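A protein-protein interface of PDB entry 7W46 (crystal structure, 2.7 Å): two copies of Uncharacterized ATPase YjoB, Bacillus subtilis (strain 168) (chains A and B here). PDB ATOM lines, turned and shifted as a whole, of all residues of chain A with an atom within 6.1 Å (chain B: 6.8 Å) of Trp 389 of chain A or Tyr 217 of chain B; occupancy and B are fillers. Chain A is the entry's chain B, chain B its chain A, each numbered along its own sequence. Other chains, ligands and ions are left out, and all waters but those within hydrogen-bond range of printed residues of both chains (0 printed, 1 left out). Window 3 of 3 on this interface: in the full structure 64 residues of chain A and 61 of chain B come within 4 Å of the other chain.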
ATOM      1  N   ARG A 352     -27.498 -30.998  12.974  1.00  0.00           N
ATOM      2  CA  ARG A 352     -26.934 -29.696  13.273  1.00  0.00           C
ATOM      3  C   ARG A 352     -25.675 -29.786  14.117  1.00  0.00           C
ATOM      4  O   ARG A 352     -24.892 -28.832  14.130  1.00  0.00           O
ATOM      5  CB  ARG A 352     -27.978 -28.831  13.977  1.00  0.00           C
ATOM      6  CG  ARG A 352     -27.650 -27.357  14.009  1.00  0.00           C
ATOM      7  CD  ARG A 352     -27.570 -26.767  12.615  1.00  0.00           C
ATOM      8  NE  ARG A 352     -27.143 -25.377  12.700  1.00  0.00           N
ATOM      9  CZ  ARG A 352     -25.873 -25.005  12.734  1.00  0.00           C
ATOM     10  NH1 ARG A 352     -24.916 -25.930  12.672  1.00  0.00           N
ATOM     11  NH2 ARG A 352     -25.555 -23.720  12.826  1.00  0.00           N
ATOM     12  N   GLY A 353     -25.470 -30.882  14.835  1.00  0.00           N
ATOM     13  CA  GLY A 353     -24.303 -31.028  15.681  1.00  0.00           C
ATOM     14  C   GLY A 353     -24.535 -30.968  17.175  1.00  0.00           C
ATOM     15  O   GLY A 353     -23.557 -30.927  17.933  1.00  0.00           O
ATOM     16  N   ILE A 356     -22.396 -33.136  19.472  1.00  0.00           N
ATOM     17  CA  ILE A 356     -21.037 -32.808  19.894  1.00  0.00           C
ATOM     18  C   ILE A 356     -20.951 -32.658  21.415  1.00  0.00           C
ATOM     19  O   ILE A 356     -19.923 -32.986  22.025  1.00  0.00           O
ATOM     20  CB  ILE A 356     -20.562 -31.524  19.174  1.00  0.00           C
ATOM     21  CG1 ILE A 356     -20.377 -31.753  17.673  1.00  0.00           C
ATOM     22  CG2 ILE A 356     -19.265 -30.999  19.759  1.00  0.00           C
ATOM     23  CD1 ILE A 356     -20.290 -30.443  16.897  1.00  0.00           C
ATOM     24  N   PHE A 357     -22.003 -32.141  22.051  1.00  0.00           N
ATOM     25  CA  PHE A 357     -21.958 -31.874  23.480  1.00  0.00           C
ATOM     26  C   PHE A 357     -23.153 -32.427  24.247  1.00  0.00           C
ATOM     27  O   PHE A 357     -23.247 -32.196  25.457  1.00  0.00           O
ATOM     28  CB  PHE A 357     -21.830 -30.361  23.746  1.00  0.00           C
ATOM     29  CG  PHE A 357     -22.815 -29.509  22.982  1.00  0.00           C
ATOM     30  CD1 PHE A 357     -24.110 -29.323  23.445  1.00  0.00           C
ATOM     31  CD2 PHE A 357     -22.432 -28.872  21.810  1.00  0.00           C
ATOM     32  CE1 PHE A 357     -25.016 -28.541  22.741  1.00  0.00           C
ATOM     33  CE2 PHE A 357     -23.335 -28.080  21.093  1.00  0.00           C
ATOM     34  CZ  PHE A 357     -24.628 -27.916  21.559  1.00  0.00           C
ATOM     35  N   TYR A 382     -28.804 -23.850  19.177  1.00  0.00           N
ATOM     36  CA  TYR A 382     -27.510 -24.468  18.900  1.00  0.00           C
ATOM     37  C   TYR A 382     -26.349 -23.504  19.130  1.00  0.00           C
ATOM     38  O   TYR A 382     -25.405 -23.812  19.865  1.00  0.00           O
ATOM     39  CB  TYR A 382     -27.482 -24.978  17.474  1.00  0.00           C
ATOM     40  CG  TYR A 382     -26.178 -25.611  17.154  1.00  0.00           C
ATOM     41  CD1 TYR A 382     -25.759 -26.741  17.837  1.00  0.00           C
ATOM     42  CD2 TYR A 382     -25.346 -25.075  16.168  1.00  0.00           C
ATOM     43  CE1 TYR A 382     -24.542 -27.336  17.540  1.00  0.00           C
ATOM     44  CE2 TYR A 382     -24.141 -25.659  15.860  1.00  0.00           C
ATOM     45  CZ  TYR A 382     -23.741 -26.792  16.548  1.00  0.00           C
ATOM     46  OH  TYR A 382     -22.533 -27.375  16.256  1.00  0.00           O
ATOM     47  N   SER A 384     -26.140 -20.845  20.811  1.00  0.00           N
ATOM     48  CA  SER A 384     -26.010 -20.398  22.193  1.00  0.00           C
ATOM     49  C   SER A 384     -25.418 -21.495  23.061  1.00  0.00           C
ATOM     50  O   SER A 384     -24.601 -21.218  23.943  1.00  0.00           O
ATOM     51  CB  SER A 384     -27.371 -19.969  22.747  1.00  0.00           C
ATOM     52  OG  SER A 384     -27.730 -18.705  22.244  1.00  0.00           O
ATOM     53  N   SER A 385     -25.855 -22.735  22.841  1.00  0.00           N
ATOM     54  CA  SER A 385     -25.291 -23.882  23.538  1.00  0.00           C
ATOM     55  C   SER A 385     -23.831 -24.087  23.169  1.00  0.00           C
ATOM     56  O   SER A 385     -22.988 -24.303  24.049  1.00  0.00           O
ATOM     57  CB  SER A 385     -26.093 -25.135  23.204  1.00  0.00           C
ATOM     58  OG  SER A 385     -27.408 -25.018  23.694  1.00  0.00           O
ATOM     59  N   ALA A 386     -23.514 -24.058  21.866  1.00  0.00           N
ATOM     60  CA  ALA A 386     -22.134 -24.273  21.442  1.00  0.00           C
ATOM     61  C   ALA A 386     -21.215 -23.226  22.044  1.00  0.00           C
ATOM     62  O   ALA A 386     -20.110 -23.550  22.488  1.00  0.00           O
ATOM     63  CB  ALA A 386     -22.045 -24.261  19.926  1.00  0.00           C
ATOM     64  N   LEU A 387     -21.670 -21.966  22.087  1.00  0.00           N
ATOM     65  CA  LEU A 387     -20.883 -20.907  22.710  1.00  0.00           C
ATOM     66  C   LEU A 387     -20.569 -21.243  24.159  1.00  0.00           C
ATOM     67  O   LEU A 387     -19.410 -21.187  24.586  1.00  0.00           O
ATOM     68  CB  LEU A 387     -21.630 -19.582  22.640  1.00  0.00           C
ATOM     69  CG  LEU A 387     -21.284 -18.640  21.504  1.00  0.00           C
ATOM     70  CD1 LEU A 387     -22.094 -17.351  21.621  1.00  0.00           C
ATOM     71  CD2 LEU A 387     -19.788 -18.369  21.511  1.00  0.00           C
ATOM     72  N   GLN A 388     -21.601 -21.596  24.929  1.00  0.00           N
ATOM     73  CA  GLN A 388     -21.417 -21.896  26.340  1.00  0.00           C
ATOM     74  C   GLN A 388     -20.583 -23.157  26.527  1.00  0.00           C
ATOM     75  O   GLN A 388     -19.729 -23.220  27.415  1.00  0.00           O
ATOM     76  CB  GLN A 388     -22.776 -22.034  27.019  1.00  0.00           C
ATOM     77  CG  GLN A 388     -22.738 -21.775  28.529  1.00  0.00           C
ATOM     78  CD  GLN A 388     -23.426 -20.470  28.930  1.00  0.00           C
ATOM     79  OE1 GLN A 388     -24.400 -20.046  28.297  1.00  0.00           O
ATOM     80  NE2 GLN A 388     -22.958 -19.858  30.020  1.00  0.00           N
ATOM     81  N   TRP A 389     -20.797 -24.166  25.684  1.00  0.00           N
ATOM     82  CA  TRP A 389     -19.951 -25.353  25.723  1.00  0.00           C
ATOM     83  C   TRP A 389     -18.496 -24.997  25.457  1.00  0.00           C
ATOM     84  O   TRP A 389     -17.611 -25.297  26.267  1.00  0.00           O
ATOM     85  CB  TRP A 389     -20.445 -26.364  24.709  1.00  0.00           C
ATOM     86  CG  TRP A 389     -19.623 -27.609  24.623  1.00  0.00           C
ATOM     87  CD1 TRP A 389     -18.733 -27.942  23.640  1.00  0.00           C
ATOM     88  CD2 TRP A 389     -19.646 -28.710  25.534  1.00  0.00           C
ATOM     89  NE1 TRP A 389     -18.194 -29.183  23.889  1.00  0.00           N
ATOM     90  CE2 TRP A 389     -18.739 -29.678  25.045  1.00  0.00           C
ATOM     91  CE3 TRP A 389     -20.348 -28.976  26.715  1.00  0.00           C
ATOM     92  CZ2 TRP A 389     -18.518 -30.893  25.697  1.00  0.00           C
ATOM     93  CZ3 TRP A 389     -20.126 -30.179  27.368  1.00  0.00           C
ATOM     94  CH2 TRP A 389     -19.219 -31.128  26.853  1.00  0.00           C
ATOM     95  N   HIS A 390     -18.233 -24.340  24.326  1.00  0.00           N
ATOM     96  CA  HIS A 390     -16.872 -23.942  23.979  1.00  0.00           C
ATOM     97  C   HIS A 390     -16.209 -23.105  25.077  1.00  0.00           C
ATOM     98  O   HIS A 390     -15.077 -23.372  25.474  1.00  0.00           O
ATOM     99  CB  HIS A 390     -16.900 -23.180  22.657  1.00  0.00           C
ATOM    100  CG  HIS A 390     -15.558 -22.752  22.168  1.00  0.00           C
ATOM    101  ND1 HIS A 390     -14.635 -23.641  21.656  1.00  0.00           N
ATOM    102  CD2 HIS A 390     -14.994 -21.527  22.079  1.00  0.00           C
ATOM    103  CE1 HIS A 390     -13.561 -22.978  21.268  1.00  0.00           C
ATOM    104  NE2 HIS A 390     -13.749 -21.695  21.522  1.00  0.00           N
ATOM    105  N   GLN A 391     -16.899 -22.087  25.584  1.00  0.00           N
ATOM    106  CA  GLN A 391     -16.258 -21.152  26.503  1.00  0.00           C
ATOM    107  C   GLN A 391     -16.255 -21.619  27.959  1.00  0.00           C
ATOM    108  O   GLN A 391     -15.444 -21.121  28.744  1.00  0.00           O
ATOM    109  CB  GLN A 391     -16.939 -19.779  26.434  1.00  0.00           C
ATOM    110  CG  GLN A 391     -16.986 -19.146  25.059  1.00  0.00           C
ATOM    111  CD  GLN A 391     -17.536 -17.728  25.092  1.00  0.00           C
ATOM    112  OE1 GLN A 391     -17.768 -17.166  26.156  1.00  0.00           O
ATOM    113  NE2 GLN A 391     -17.732 -17.146  23.926  1.00  0.00           N
ATOM    114  N   GLU A 392     -17.127 -22.549  28.348  1.00  0.00           N
ATOM    115  CA  GLU A 392     -17.257 -22.875  29.766  1.00  0.00           C
ATOM    116  C   GLU A 392     -17.358 -24.362  30.102  1.00  0.00           C
ATOM    117  O   GLU A 392     -17.263 -24.701  31.286  1.00  0.00           O
ATOM    118  CB  GLU A 392     -18.466 -22.123  30.370  1.00  0.00           C
ATOM    119  CG  GLU A 392     -18.159 -20.607  30.689  1.00  0.00           C
ATOM    120  CD  GLU A 392     -19.428 -19.700  30.790  1.00  0.00           C
ATOM    121  OE1 GLU A 392     -19.622 -18.799  29.918  1.00  0.00           O
ATOM    122  OE2 GLU A 392     -20.220 -19.869  31.769  1.00  0.00           O
ATOM    123  N   GLY A 393     -17.515 -25.264  29.143  1.00  0.00           N
ATOM    124  CA  GLY A 393     -17.559 -26.670  29.464  1.00  0.00           C
ATOM    125  C   GLY A 393     -18.893 -27.192  29.937  1.00  0.00           C
ATOM    126  O   GLY A 393     -19.037 -28.414  30.106  1.00  0.00           O
ATOM    127  N   ASN A 394     -19.859 -26.318  30.183  1.00  0.00           N
ATOM    128  CA  ASN A 394     -21.241 -26.676  30.466  1.00  0.00           C
ATOM    129  C   ASN A 394     -22.064 -26.392  29.213  1.00  0.00           C
ATOM    130  O   ASN A 394     -21.584 -25.737  28.296  1.00  0.00           O
ATOM    131  CB  ASN A 394     -21.757 -25.891  31.686  1.00  0.00           C
ATOM    132  CG  ASN A 394     -22.039 -24.408  31.379  1.00  0.00           C
ATOM    133  OD1 ASN A 394     -22.607 -24.057  30.337  1.00  0.00           O
ATOM    134  ND2 ASN A 394     -21.633 -23.530  32.297  1.00  0.00           N
ATOM    135  N   HIS A 395     -23.327 -26.823  29.188  1.00  0.00           N
ATOM    136  CA  HIS A 395     -24.133 -26.395  28.045  1.00  0.00           C
ATOM    137  C   HIS A 395     -25.414 -25.658  28.436  1.00  0.00           C
ATOM    138  O   HIS A 395     -25.859 -24.775  27.689  1.00  0.00           O
ATOM    139  CB  HIS A 395     -24.471 -27.582  27.124  1.00  0.00           C
ATOM    140  CG  HIS A 395     -24.849 -28.845  27.841  1.00  0.00           C
ATOM    141  ND1 HIS A 395     -26.048 -28.999  28.501  1.00  0.00           N
ATOM    142  CD2 HIS A 395     -24.200 -30.027  27.963  1.00  0.00           C
ATOM    143  CE1 HIS A 395     -26.114 -30.213  29.018  1.00  0.00           C
ATOM    144  NE2 HIS A 395     -25.004 -30.858  28.705  1.00  0.00           N
ATOM    145  N   SER B 212     -11.631 -20.284  14.713  1.00  0.00           N
ATOM    146  CA  SER B 212     -11.868 -21.692  14.403  1.00  0.00           C
ATOM    147  C   SER B 212     -13.207 -22.182  14.956  1.00  0.00           C
ATOM    148  O   SER B 212     -13.805 -23.111  14.400  1.00  0.00           O
ATOM    149  CB  SER B 212     -10.705 -22.538  14.934  1.00  0.00           C
ATOM    150  OG  SER B 212     -10.701 -22.599  16.351  1.00  0.00           O
ATOM    151  N   PHE B 213     -13.690 -21.567  16.039  1.00  0.00           N
ATOM    152  CA  PHE B 213     -14.985 -21.923  16.605  1.00  0.00           C
ATOM    153  C   PHE B 213     -16.069 -22.056  15.535  1.00  0.00           C
ATOM    154  O   PHE B 213     -16.811 -23.045  15.507  1.00  0.00           O
ATOM    155  CB  PHE B 213     -15.388 -20.884  17.647  1.00  0.00           C
ATOM    156  CG  PHE B 213     -16.825 -20.959  18.042  1.00  0.00           C
ATOM    157  CD1 PHE B 213     -17.249 -21.885  18.986  1.00  0.00           C
ATOM    158  CD2 PHE B 213     -17.761 -20.110  17.463  1.00  0.00           C
ATOM    159  CE1 PHE B 213     -18.579 -21.961  19.365  1.00  0.00           C
ATOM    160  CE2 PHE B 213     -19.106 -20.190  17.824  1.00  0.00           C
ATOM    161  CZ  PHE B 213     -19.515 -21.124  18.782  1.00  0.00           C
ATOM    162  N   TYR B 214     -16.186 -21.065  14.646  1.00  0.00           N
ATOM    163  CA  TYR B 214     -17.275 -21.087  13.673  1.00  0.00           C
ATOM    164  C   TYR B 214     -17.153 -22.276  12.735  1.00  0.00           C
ATOM    165  O   TYR B 214     -18.164 -22.808  12.271  1.00  0.00           O
ATOM    166  CB  TYR B 214     -17.328 -19.739  12.924  1.00  0.00           C
ATOM    167  CG  TYR B 214     -17.691 -18.642  13.905  1.00  0.00           C
ATOM    168  CD1 TYR B 214     -16.716 -17.997  14.660  1.00  0.00           C
ATOM    169  CD2 TYR B 214     -19.024 -18.342  14.172  1.00  0.00           C
ATOM    170  CE1 TYR B 214     -17.063 -17.039  15.601  1.00  0.00           C
ATOM    171  CE2 TYR B 214     -19.371 -17.407  15.117  1.00  0.00           C
ATOM    172  CZ  TYR B 214     -18.394 -16.759  15.824  1.00  0.00           C
ATOM    173  OH  TYR B 214     -18.772 -15.824  16.751  1.00  0.00           O
ATOM    174  N   GLN B 215     -15.929 -22.723  12.469  1.00  0.00           N
ATOM    175  CA  GLN B 215     -15.728 -23.900  11.629  1.00  0.00           C
ATOM    176  C   GLN B 215     -16.025 -25.187  12.396  1.00  0.00           C
ATOM    177  O   GLN B 215     -16.663 -26.100  11.866  1.00  0.00           O
ATOM    178  CB  GLN B 215     -14.299 -23.913  11.083  1.00  0.00           C
ATOM    179  CG  GLN B 215     -14.080 -24.928   9.968  1.00  0.00           C
ATOM    180  CD  GLN B 215     -12.647 -24.942   9.427  1.00  0.00           C
ATOM    181  OE1 GLN B 215     -11.709 -25.380  10.108  1.00  0.00           O
ATOM    182  NE2 GLN B 215     -12.479 -24.474   8.193  1.00  0.00           N
ATOM    183  N   THR B 216     -15.605 -25.250  13.655  1.00  0.00           N
ATOM    184  CA  THR B 216     -15.795 -26.446  14.465  1.00  0.00           C
ATOM    185  C   THR B 216     -17.274 -26.811  14.610  1.00  0.00           C
ATOM    186  O   THR B 216     -17.669 -27.965  14.395  1.00  0.00           O
ATOM    187  CB  THR B 216     -15.156 -26.212  15.831  1.00  0.00           C
ATOM    188  OG1 THR B 216     -13.761 -25.984  15.656  1.00  0.00           O
ATOM    189  CG2 THR B 216     -15.332 -27.403  16.722  1.00  0.00           C
ATOM    190  N   TYR B 217     -18.106 -25.853  15.021  1.00  0.00           N
ATOM    191  CA  TYR B 217     -19.525 -26.108  15.255  1.00  0.00           C
ATOM    192  C   TYR B 217     -20.361 -25.815  14.027  1.00  0.00           C
ATOM    193  O   TYR B 217     -21.585 -25.964  14.082  1.00  0.00           O
ATOM    194  CB  TYR B 217     -19.994 -25.303  16.468  1.00  0.00           C
ATOM    195  CG  TYR B 217     -19.191 -25.717  17.679  1.00  0.00           C
ATOM    196  CD1 TYR B 217     -19.526 -26.857  18.394  1.00  0.00           C
ATOM    197  CD2 TYR B 217     -18.048 -25.035  18.054  1.00  0.00           C
ATOM    198  CE1 TYR B 217     -18.779 -27.278  19.470  1.00  0.00           C
ATOM    199  CE2 TYR B 217     -17.291 -25.453  19.148  1.00  0.00           C
ATOM    200  CZ  TYR B 217     -17.663 -26.583  19.846  1.00  0.00           C
ATOM    201  OH  TYR B 217     -16.919 -27.014  20.925  1.00  0.00           O
ATOM    202  N   ASP B 218     -19.708 -25.458  12.915  1.00  0.00           N
ATOM    203  CA  ASP B 218     -20.344 -25.114  11.643  1.00  0.00           C
ATOM    204  C   ASP B 218     -21.467 -24.088  11.832  1.00  0.00           C
ATOM    205  O   ASP B 218     -22.659 -24.389  11.701  1.00  0.00           O
ATOM    206  CB  ASP B 218     -20.867 -26.374  10.951  1.00  0.00           C
ATOM    207  CG  ASP B 218     -21.355 -26.098   9.544  1.00  0.00           C
ATOM    208  OD1 ASP B 218     -20.929 -25.095   8.932  1.00  0.00           O
ATOM    209  OD2 ASP B 218     -22.189 -26.891   9.050  1.00  0.00           O
ATOM    210  N   ILE B 219     -21.060 -22.857  12.137  1.00  0.00           N
ATOM    211  CA  ILE B 219     -21.977 -21.796  12.514  1.00  0.00           C
ATOM    212  C   ILE B 219     -21.716 -20.583  11.601  1.00  0.00           C
ATOM    213  O   ILE B 219     -20.557 -20.231  11.404  1.00  0.00           O
ATOM    214  CB  ILE B 219     -21.844 -21.398  13.989  1.00  0.00           C
ATOM    215  CG1 ILE B 219     -22.343 -22.555  14.857  1.00  0.00           C
ATOM    216  CG2 ILE B 219     -22.607 -20.137  14.305  1.00  0.00           C
ATOM    217  CD1 ILE B 219     -22.084 -22.373  16.321  1.00  0.00           C
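The side-chain hydroxyl (OH) of Tyr 382 of chain A sits at hydrogen-bond distance from the backbone carbonyl oxygen (O) of Tyr 217 of chain B, at 2.8 Å. The guanidinium group (NH1) of Arg 352 of chain A is in hydrogen-bond range of the backbone carbonyl oxygen (O) of Asp 218 of chain B (2.9 Å).
The backbone carbonyl oxygen (O) of Arg 352 of chain A lies close to the side-chain hydroxyl (OH) of Tyr 382 of chain A (3.5 Å). O of Tyr 214 of chain B sits at hydrogen-bond distance from N of Ile 219 of chain B (2.9 Å). The backbone NH (N) of Trp 389 of chain A sits close to the backbone carbonyl oxygen (O) of Asn 394 of chain A.
Among the printed residues, pairs that only touch across the chains: Trp 389 of chain A with Tyr 217 of chain B, Arg 352 of chain A with Tyr 217 of chain B, His 390 of chain A with Phe 213 of chain B, Tyr 382 of chain A with Ile 219 of chain B, Ile 356 of chain A with Tyr 217 of chain B, Ala 386 of chain A with Phe 213 of chain B, Leu 387 of chain A with Phe 213 of chain B, Ala 386 of chain A with Tyr 217 of chain B and Arg 352 of chain A with Ile 219 of chain B.
Trp 389 of chain A touches just one residue of chain B: Tyr 217. Tyr 217 of chain B touches just these residues of chain A: Arg 352, Ile 356, Tyr 382, Ala 386 and Trp 389. Printed residues of chain B within 4 Å of Tyr 382 of chain A: Tyr 217 and Ile 219. Printed residues of chain B within 4 Å of Ile 356 of chain A: Tyr 217. Of the printed residues of chain A, Phe 213 of chain B touches Ala 386 (3.8 Å), Leu 387 (3.9 Å) and His 390 (3.7 Å). Of the printed residues of chain B, Arg 352 of chain A touches Tyr 217 (3.6 Å), Asp 218 (2.9 Å) and Ile 219 (3.97 Å). Asn 394 of chain A touches none of the printed residues of chain B. Glu 392 of chain A touches none of the printed residues of chain B. The nearest printed residue of chain B that does not touch Trp 389 of chain A is Phe 213 of chain B (6.8 Å).
Printed residues of chain B that touch a printed residue of chain A: Phe 213, Tyr 217, Asp 218 and Ile 219. Hydrophobic or aromatic side chains of chain B within 4 Å of the printed part of chain A: Phe 213, Tyr 217 and Ile 219. Along chain A the printed residues that touch a printed residue of chain B span positions 352 to 390. Among the printed residues, 11 pairs touch across the chains. Among the printed residues, no Asp or Glu carboxylate lies within 4 Å of a Lys or Arg side-chain nitrogen of the other chain.
No position is printed for both chains.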
